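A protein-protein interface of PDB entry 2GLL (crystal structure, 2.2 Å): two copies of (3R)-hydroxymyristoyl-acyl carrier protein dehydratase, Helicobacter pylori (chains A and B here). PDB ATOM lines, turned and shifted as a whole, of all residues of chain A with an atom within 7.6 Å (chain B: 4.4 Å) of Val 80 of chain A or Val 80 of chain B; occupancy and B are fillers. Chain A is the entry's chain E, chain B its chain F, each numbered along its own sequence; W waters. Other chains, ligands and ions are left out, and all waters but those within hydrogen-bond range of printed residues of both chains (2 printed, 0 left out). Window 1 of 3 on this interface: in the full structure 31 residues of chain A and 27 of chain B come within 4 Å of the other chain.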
ATOM      1  N   MET A  39     -24.917   8.748  32.630  1.00  0.00           N
ATOM      2  CA  MET A  39     -23.909   7.848  32.100  1.00  0.00           C
ATOM      3  C   MET A  39     -22.734   7.552  33.044  1.00  0.00           C
ATOM      4  O   MET A  39     -21.683   7.072  32.614  1.00  0.00           O
ATOM      5  CB  MET A  39     -23.409   8.409  30.770  1.00  0.00           C
ATOM      6  CG  MET A  39     -23.118   7.365  29.706  1.00  0.00           C
ATOM      7  SD  MET A  39     -24.499   6.249  29.308  1.00  0.00           S
ATOM      8  CE  MET A  39     -23.619   4.760  29.156  1.00  0.00           C
ATOM      9  N   LEU A  41     -21.851   5.170  35.722  1.00  0.00           N
ATOM     10  CA  LEU A  41     -22.326   3.888  36.234  1.00  0.00           C
ATOM     11  C   LEU A  41     -21.449   3.185  37.279  1.00  0.00           C
ATOM     12  O   LEU A  41     -21.360   1.958  37.310  1.00  0.00           O
ATOM     13  CB  LEU A  41     -22.580   2.947  35.044  1.00  0.00           C
ATOM     14  CG  LEU A  41     -23.324   3.594  33.855  1.00  0.00           C
ATOM     15  CD1 LEU A  41     -23.398   2.616  32.684  1.00  0.00           C
ATOM     16  CD2 LEU A  41     -24.726   4.034  34.286  1.00  0.00           C
ATOM     17  N   HIS A  70     -36.334  -0.886  28.878  1.00  0.00           N
ATOM     18  CA  HIS A  70     -35.579  -2.129  28.809  1.00  0.00           C
ATOM     19  C   HIS A  70     -35.880  -3.099  29.955  1.00  0.00           C
ATOM     20  O   HIS A  70     -35.047  -3.258  30.842  1.00  0.00           O
ATOM     21  CB  HIS A  70     -34.082  -1.802  28.810  1.00  0.00           C
ATOM     22  CG  HIS A  70     -33.203  -2.936  28.381  1.00  0.00           C
ATOM     23  ND1 HIS A  70     -32.727  -3.063  27.092  1.00  0.00           N
ATOM     24  CD2 HIS A  70     -32.703  -3.988  29.069  1.00  0.00           C
ATOM     25  CE1 HIS A  70     -31.972  -4.142  27.007  1.00  0.00           C
ATOM     26  NE2 HIS A  70     -31.941  -4.722  28.194  1.00  0.00           N
ATOM     27  N   PHE A  77     -31.290  -4.769  33.551  1.00  0.00           N
ATOM     28  CA  PHE A  77     -30.212  -3.807  33.355  1.00  0.00           C
ATOM     29  C   PHE A  77     -29.467  -4.185  32.069  1.00  0.00           C
ATOM     30  O   PHE A  77     -28.916  -5.275  31.968  1.00  0.00           O
ATOM     31  CB  PHE A  77     -29.257  -3.829  34.549  1.00  0.00           C
ATOM     32  CG  PHE A  77     -28.274  -2.687  34.559  1.00  0.00           C
ATOM     33  CD1 PHE A  77     -28.708  -1.383  34.762  1.00  0.00           C
ATOM     34  CD2 PHE A  77     -26.916  -2.916  34.358  1.00  0.00           C
ATOM     35  CE1 PHE A  77     -27.808  -0.328  34.765  1.00  0.00           C
ATOM     36  CE2 PHE A  77     -26.009  -1.868  34.360  1.00  0.00           C
ATOM     37  CZ  PHE A  77     -26.456  -0.570  34.564  1.00  0.00           C
ATOM     38  N   PRO A  78     -29.433  -3.281  31.077  1.00  0.00           N
ATOM     39  CA  PRO A  78     -28.754  -3.552  29.801  1.00  0.00           C
ATOM     40  C   PRO A  78     -27.345  -4.133  29.939  1.00  0.00           C
ATOM     41  O   PRO A  78     -26.530  -3.641  30.723  1.00  0.00           O
ATOM     42  CB  PRO A  78     -28.754  -2.185  29.112  1.00  0.00           C
ATOM     43  CG  PRO A  78     -29.980  -1.517  29.663  1.00  0.00           C
ATOM     44  CD  PRO A  78     -29.900  -1.882  31.130  1.00  0.00           C
ATOM     45  N   GLY A  79     -27.076  -5.187  29.170  1.00  0.00           N
ATOM     46  CA  GLY A  79     -25.779  -5.834  29.194  1.00  0.00           C
ATOM     47  C   GLY A  79     -24.652  -4.903  28.787  1.00  0.00           C
ATOM     48  O   GLY A  79     -23.585  -4.919  29.403  1.00  0.00           O
ATOM     49  N   VAL A  80     -24.881  -4.085  27.761  1.00  0.00           N
ATOM     50  CA  VAL A  80     -23.861  -3.154  27.295  1.00  0.00           C
ATOM     51  C   VAL A  80     -23.530  -2.088  28.335  1.00  0.00           C
ATOM     52  O   VAL A  80     -22.468  -1.473  28.274  1.00  0.00           O
ATOM     53  CB  VAL A  80     -24.266  -2.450  25.973  1.00  0.00           C
ATOM     54  CG1 VAL A  80     -24.395  -3.471  24.862  1.00  0.00           C
ATOM     55  CG2 VAL A  80     -25.561  -1.675  26.150  1.00  0.00           C
ATOM     56  N   LEU A  81     -24.429  -1.865  29.292  1.00  0.00           N
ATOM     57  CA  LEU A  81     -24.160  -0.875  30.328  1.00  0.00           C
ATOM     58  C   LEU A  81     -23.329  -1.489  31.448  1.00  0.00           C
ATOM     59  O   LEU A  81     -22.692  -0.772  32.216  1.00  0.00           O
ATOM     60  CB  LEU A  81     -25.458  -0.275  30.887  1.00  0.00           C
ATOM     61  CG  LEU A  81     -26.242   0.626  29.920  1.00  0.00           C
ATOM     62  CD1 LEU A  81     -27.245   1.467  30.698  1.00  0.00           C
ATOM     63  CD2 LEU A  81     -25.290   1.539  29.153  1.00  0.00           C
ATOM     64  N   ILE A  82     -23.337  -2.816  31.541  1.00  0.00           N
ATOM     65  CA  ILE A  82     -22.533  -3.513  32.547  1.00  0.00           C
ATOM     66  C   ILE A  82     -21.086  -3.378  32.067  1.00  0.00           C
ATOM     67  O   ILE A  82     -20.171  -3.125  32.851  1.00  0.00           O
ATOM     68  CB  ILE A  82     -22.909  -5.010  32.637  1.00  0.00           C
ATOM     69  CG1 ILE A  82     -24.373  -5.151  33.049  1.00  0.00           C
ATOM     70  CG2 ILE A  82     -22.001  -5.718  33.635  1.00  0.00           C
ATOM     71  CD1 ILE A  82     -24.851  -6.585  33.206  1.00  0.00           C
ATOM     72  N   VAL A  83     -20.904  -3.528  30.759  1.00  0.00           N
ATOM     73  CA  VAL A  83     -19.593  -3.404  30.132  1.00  0.00           C
ATOM     74  C   VAL A  83     -19.092  -1.979  30.315  1.00  0.00           C
ATOM     75  O   VAL A  83     -17.908  -1.750  30.561  1.00  0.00           O
ATOM     76  CB  VAL A  83     -19.675  -3.713  28.628  1.00  0.00           C
ATOM     77  CG1 VAL A  83     -18.331  -3.440  27.961  1.00  0.00           C
ATOM     78  CG2 VAL A  83     -20.093  -5.157  28.429  1.00  0.00           C
ATOM     79  N   GLU A  84     -20.015  -1.030  30.194  1.00  0.00           N
ATOM     80  CA  GLU A  84     -19.720   0.385  30.349  1.00  0.00           C
ATOM     81  C   GLU A  84     -19.257   0.648  31.779  1.00  0.00           C
ATOM     82  O   GLU A  84     -18.314   1.406  32.003  1.00  0.00           O
ATOM     83  CB  GLU A  84     -20.978   1.213  30.034  1.00  0.00           C
ATOM     84  CG  GLU A  84     -20.853   2.726  30.240  1.00  0.00           C
ATOM     85  CD  GLU A  84     -19.775   3.366  29.370  1.00  0.00           C
ATOM     86  OE1 GLU A  84     -19.686   3.018  28.176  1.00  0.00           O
ATOM     87  OE2 GLU A  84     -19.028   4.226  29.873  1.00  0.00           O
ATOM     88  N   GLY A  85     -19.928   0.017  32.740  1.00  0.00           N
ATOM     89  CA  GLY A  85     -19.572   0.182  34.141  1.00  0.00           C
ATOM     90  C   GLY A  85     -18.210  -0.420  34.462  1.00  0.00           C
ATOM     91  O   GLY A  85     -17.493   0.068  35.342  1.00  0.00           O
ATOM     92  N   MET A  86     -17.845  -1.478  33.745  1.00  0.00           N
ATOM     93  CA  MET A  86     -16.559  -2.126  33.956  1.00  0.00           C
ATOM     94  C   MET A  86     -15.463  -1.227  33.401  1.00  0.00           C
ATOM     95  O   MET A  86     -14.386  -1.101  33.986  1.00  0.00           O
ATOM     96  CB  MET A  86     -16.539  -3.487  33.257  1.00  0.00           C
ATOM     97  CG  MET A  86     -17.518  -4.494  33.856  1.00  0.00           C
ATOM     98  SD  MET A  86     -17.618  -6.046  32.931  1.00  0.00           S
ATOM     99  CE  MET A  86     -16.091  -6.863  33.449  1.00  0.00           C
ATOM    100  N   ALA A  87     -15.760  -0.589  32.272  1.00  0.00           N
ATOM    101  CA  ALA A  87     -14.820   0.310  31.616  1.00  0.00           C
ATOM    102  C   ALA A  87     -14.536   1.532  32.482  1.00  0.00           C
ATOM    103  O   ALA A  87     -13.396   1.985  32.585  1.00  0.00           O
ATOM    104  CB  ALA A  87     -15.375   0.743  30.270  1.00  0.00           C
ATOM    105  N   PHE A 113     -13.456   4.428  24.246  1.00  0.00           N
ATOM    106  CA  PHE A 113     -13.430   2.979  24.180  1.00  0.00           C
ATOM    107  C   PHE A 113     -12.622   2.684  22.921  1.00  0.00           C
ATOM    108  O   PHE A 113     -12.761   3.389  21.927  1.00  0.00           O
ATOM    109  CB  PHE A 113     -14.850   2.447  23.994  1.00  0.00           C
ATOM    110  CG  PHE A 113     -15.322   1.571  25.102  1.00  0.00           C
ATOM    111  CD1 PHE A 113     -14.739   0.325  25.315  1.00  0.00           C
ATOM    112  CD2 PHE A 113     -16.350   1.990  25.942  1.00  0.00           C
ATOM    113  CE1 PHE A 113     -15.180  -0.499  26.356  1.00  0.00           C
ATOM    114  CE2 PHE A 113     -16.796   1.176  26.982  1.00  0.00           C
ATOM    115  CZ  PHE A 113     -16.208  -0.072  27.188  1.00  0.00           C
ATOM    116  N   ILE A 116     -13.510  -4.069  22.574  1.00  0.00           N
ATOM    117  CA  ILE A 116     -14.248  -4.871  23.536  1.00  0.00           C
ATOM    118  C   ILE A 116     -14.193  -6.304  23.029  1.00  0.00           C
ATOM    119  O   ILE A 116     -14.567  -6.572  21.889  1.00  0.00           O
ATOM    120  CB  ILE A 116     -15.716  -4.425  23.633  1.00  0.00           C
ATOM    121  CG1 ILE A 116     -15.781  -2.962  24.077  1.00  0.00           C
ATOM    122  CG2 ILE A 116     -16.462  -5.302  24.627  1.00  0.00           C
ATOM    123  CD1 ILE A 116     -17.178  -2.440  24.244  1.00  0.00           C
ATOM    124  N   VAL A 119     -16.790 -10.885  25.706  1.00  0.00           N
ATOM    125  CA  VAL A 119     -17.757 -10.580  26.758  1.00  0.00           C
ATOM    126  C   VAL A 119     -18.812 -11.674  26.756  1.00  0.00           C
ATOM    127  O   VAL A 119     -19.178 -12.200  25.713  1.00  0.00           O
ATOM    128  CB  VAL A 119     -18.450  -9.191  26.587  1.00  0.00           C
ATOM    129  CG1 VAL A 119     -17.551  -8.245  25.832  1.00  0.00           C
ATOM    130  CG2 VAL A 119     -19.794  -9.344  25.919  1.00  0.00           C
ATOM    131  N   PHE A 121     -22.523 -12.751  28.967  1.00  0.00           N
ATOM    132  CA  PHE A 121     -23.516 -12.483  30.008  1.00  0.00           C
ATOM    133  C   PHE A 121     -24.088 -13.826  30.447  1.00  0.00           C
ATOM    134  O   PHE A 121     -24.506 -14.625  29.614  1.00  0.00           O
ATOM    135  CB  PHE A 121     -24.627 -11.565  29.469  1.00  0.00           C
ATOM    136  CG  PHE A 121     -24.110 -10.308  28.821  1.00  0.00           C
ATOM    137  CD1 PHE A 121     -23.979 -10.223  27.440  1.00  0.00           C
ATOM    138  CD2 PHE A 121     -23.707  -9.229  29.595  1.00  0.00           C
ATOM    139  CE1 PHE A 121     -23.450  -9.079  26.840  1.00  0.00           C
ATOM    140  CE2 PHE A 121     -23.176  -8.082  29.004  1.00  0.00           C
ATOM    141  CZ  PHE A 121     -23.047  -8.011  27.626  1.00  0.00           C
ATOM    142  N   PRO B  78     -22.083   7.044  23.004  1.00  0.00           N
ATOM    143  CA  PRO B  78     -21.425   5.904  23.656  1.00  0.00           C
ATOM    144  C   PRO B  78     -21.167   4.695  22.753  1.00  0.00           C
ATOM    145  O   PRO B  78     -22.072   4.203  22.075  1.00  0.00           O
ATOM    146  CB  PRO B  78     -22.371   5.577  24.816  1.00  0.00           C
ATOM    147  CG  PRO B  78     -22.940   6.900  25.164  1.00  0.00           C
ATOM    148  CD  PRO B  78     -23.243   7.487  23.794  1.00  0.00           C
ATOM    149  N   GLY B  79     -19.927   4.221  22.760  1.00  0.00           N
ATOM    150  CA  GLY B  79     -19.566   3.070  21.947  1.00  0.00           C
ATOM    151  C   GLY B  79     -20.413   1.848  22.247  1.00  0.00           C
ATOM    152  O   GLY B  79     -20.748   1.080  21.348  1.00  0.00           O
ATOM    153  N   VAL B  80     -20.766   1.667  23.515  1.00  0.00           N
ATOM    154  CA  VAL B  80     -21.580   0.534  23.906  1.00  0.00           C
ATOM    155  C   VAL B  80     -22.987   0.645  23.328  1.00  0.00           C
ATOM    156  O   VAL B  80     -23.643  -0.366  23.077  1.00  0.00           O
ATOM    157  CB  VAL B  80     -21.661   0.407  25.441  1.00  0.00           C
ATOM    158  CG1 VAL B  80     -20.275   0.203  26.019  1.00  0.00           C
ATOM    159  CG2 VAL B  80     -22.324   1.638  26.035  1.00  0.00           C
ATOM    160  N   LEU B  81     -23.452   1.872  23.106  1.00  0.00           N
ATOM    161  CA  LEU B  81     -24.787   2.068  22.551  1.00  0.00           C
ATOM    162  C   LEU B  81     -24.762   1.822  21.046  1.00  0.00           C
ATOM    163  O   LEU B  81     -25.784   1.479  20.455  1.00  0.00           O
ATOM    164  CB  LEU B  81     -25.320   3.466  22.880  1.00  0.00           C
ATOM    165  CG  LEU B  81     -25.592   3.705  24.375  1.00  0.00           C
ATOM    166  CD1 LEU B  81     -26.357   5.015  24.554  1.00  0.00           C
ATOM    167  CD2 LEU B  81     -26.400   2.540  24.955  1.00  0.00           C
ATOM    168  N   ILE B  82     -23.592   1.991  20.434  1.00  0.00           N
ATOM    169  CA  ILE B  82     -23.459   1.713  19.009  1.00  0.00           C
ATOM    170  C   ILE B  82     -23.628   0.200  18.907  1.00  0.00           C
ATOM    171  O   ILE B  82     -24.352  -0.301  18.049  1.00  0.00           O
ATOM    172  CB  ILE B  82     -22.061   2.088  18.457  1.00  0.00           C
ATOM    173  CG1 ILE B  82     -21.825   3.593  18.595  1.00  0.00           C
ATOM    174  CG2 ILE B  82     -21.948   1.672  16.989  1.00  0.00           C
ATOM    175  CD1 ILE B  82     -20.533   4.062  17.985  1.00  0.00           C
ATOM    176  N   VAL B  83     -22.964  -0.522  19.807  1.00  0.00           N
ATOM    177  CA  VAL B  83     -23.055  -1.976  19.821  1.00  0.00           C
ATOM    178  C   VAL B  83     -24.499  -2.411  20.087  1.00  0.00           C
ATOM    179  O   VAL B  83     -25.004  -3.322  19.440  1.00  0.00           O
ATOM    180  CB  VAL B  83     -22.114  -2.602  20.900  1.00  0.00           C
ATOM    181  CG1 VAL B  83     -22.245  -4.132  20.897  1.00  0.00           C
ATOM    182  CG2 VAL B  83     -20.669  -2.220  20.617  1.00  0.00           C
ATOM    183  N   GLU B  84     -25.159  -1.757  21.035  1.00  0.00           N
ATOM    184  CA  GLU B  84     -26.551  -2.080  21.354  1.00  0.00           C
ATOM    185  C   GLU B  84     -27.412  -1.894  20.094  1.00  0.00           C
ATOM    186  O   GLU B  84     -28.318  -2.682  19.813  1.00  0.00           O
ATOM    187  CB  GLU B  84     -27.041  -1.164  22.487  1.00  0.00           C
ATOM    188  CG  GLU B  84     -28.497  -1.337  22.915  1.00  0.00           C
ATOM    189  CD  GLU B  84     -28.833  -2.733  23.433  1.00  0.00           C
ATOM    190  OE1 GLU B  84     -27.982  -3.374  24.095  1.00  0.00           O
ATOM    191  OE2 GLU B  84     -29.969  -3.184  23.196  1.00  0.00           O
ATOM    192  N   PHE B 113     -28.673 -10.360  25.761  1.00  0.00           N
ATOM    193  CA  PHE B 113     -27.352 -10.363  25.160  1.00  0.00           C
ATOM    194  C   PHE B 113     -26.653 -11.605  25.703  1.00  0.00           C
ATOM    195  O   PHE B 113     -26.751 -11.883  26.894  1.00  0.00           O
ATOM    196  CB  PHE B 113     -26.586  -9.113  25.583  1.00  0.00           C
ATOM    197  CG  PHE B 113     -26.225  -8.209  24.444  1.00  0.00           C
ATOM    198  CD1 PHE B 113     -26.881  -6.990  24.269  1.00  0.00           C
ATOM    199  CD2 PHE B 113     -25.217  -8.568  23.554  1.00  0.00           C
ATOM    200  CE1 PHE B 113     -26.530  -6.137  23.224  1.00  0.00           C
ATOM    201  CE2 PHE B 113     -24.860  -7.726  22.508  1.00  0.00           C
ATOM    202  CZ  PHE B 113     -25.516  -6.508  22.343  1.00  0.00           C
ATOM    203  N   ILE B 116     -20.433 -10.855  23.134  1.00  0.00           N
ATOM    204  CA  ILE B 116     -20.043  -9.731  22.285  1.00  0.00           C
ATOM    205  C   ILE B 116     -18.552  -9.937  22.092  1.00  0.00           C
ATOM    206  O   ILE B 116     -17.840 -10.222  23.060  1.00  0.00           O
ATOM    207  CB  ILE B 116     -20.218  -8.365  22.977  1.00  0.00           C
ATOM    208  CG1 ILE B 116     -21.651  -8.194  23.487  1.00  0.00           C
ATOM    209  CG2 ILE B 116     -19.879  -7.256  21.989  1.00  0.00           C
ATOM    210  CD1 ILE B 116     -21.835  -6.981  24.401  1.00  0.00           C
HETATM  211  O   HOH W   1     -27.779  -4.181  26.590  1.00  0.00           O
HETATM  212  O   HOH W   2     -19.446   3.602  25.691  1.00  0.00           O
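Water W2 lies within hydrogen-bond range of OE1 of Glu 84 of chain A, N of Gly 79 of chain B and N of Val 80 of chain B.
Water W1 lies within hydrogen-bond range of OE1 of Glu 84 of chain B, N of Gly 79 of chain A and N of Val 80 of chain A.
CB of Val 80 of chain B touches O of Val 80 of chain A, at 3.5 Å.
CG2 of Val 80 of chain A touches OE1 of Glu 84 of chain B, 3.6 Å away.
Phe 113 of chain B touches Val 80 of chain A.
Val 80 of chain B touches Glu 84 of chain A (CG1 to OE1, 3.6 Å).
CG1 of Val 80 of chain B touches CE2 of Phe 113 of chain A, at 3.7 Å.
Phe 113 of chain B touches Phe 121 of chain A (O to CD1, 3.3 Å).
Phe 121 of chain A touches Ile 116 of chain B (CZ to CD1, 3.6 Å).
The backbone NH (N) of Val 119 of chain A is in hydrogen-bond range of the backbone carbonyl oxygen (O) of Ile 116 of chain B, at 2.9 Å.
His 70 of chain A touches none of the printed residues of chain B.
Gly 79 of chain A touches none of the printed residues of chain B.
Of chain B, only Val 80 (3.5 Å), Glu 84 (3.6 Å) and Phe 113 (3.8 Å) come within 4 Å of Val 80 of chain A.
Of the printed residues of chain B, Glu 84 of chain A touches Val 80 (3.6 Å).
Of the printed residues of chain B, Phe 113 of chain A touches Val 80.
No residue of chain A comes within 4 Å of Gly 79 of chain B.
Val 80 of chain B touches just these residues of chain A: Val 80 (3.5 Å), Glu 84 (3.6 Å) and Phe 113 (3.7 Å).
Of the printed residues of chain A, Glu 84 of chain B touches Val 80 (3.6 Å).
Of the printed residues of chain A, Phe 113 of chain B touches Val 80 and Phe 121.
Of the printed residues of chain A, Ile 116 of chain B touches Val 119 and Phe 121.
The nearest printed residue of chain B that does not touch Val 80 of chain A is Ile 116 of chain B (4.4 Å).
Of the 18 printed residues of chain A, 5 touch a printed residue of chain B.
Among the printed residues, 8 pairs touch across the chains.
Among the printed residues, no Asp or Glu carboxylate lies within 4 Å of a Lys or Arg side-chain nitrogen of the other chain.
Val 80 of chain B touches its own counterpart, Val 80 of chain A.
Val 80 of chain A touches Glu 84 of chain B, and with the chains exchanged Glu 84 of chain A touches Val 80 of chain B.
Val 80 of chain A touches Phe 113 of chain B, and with the chains exchanged Phe 113 of chain A touches Val 80 of chain B.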
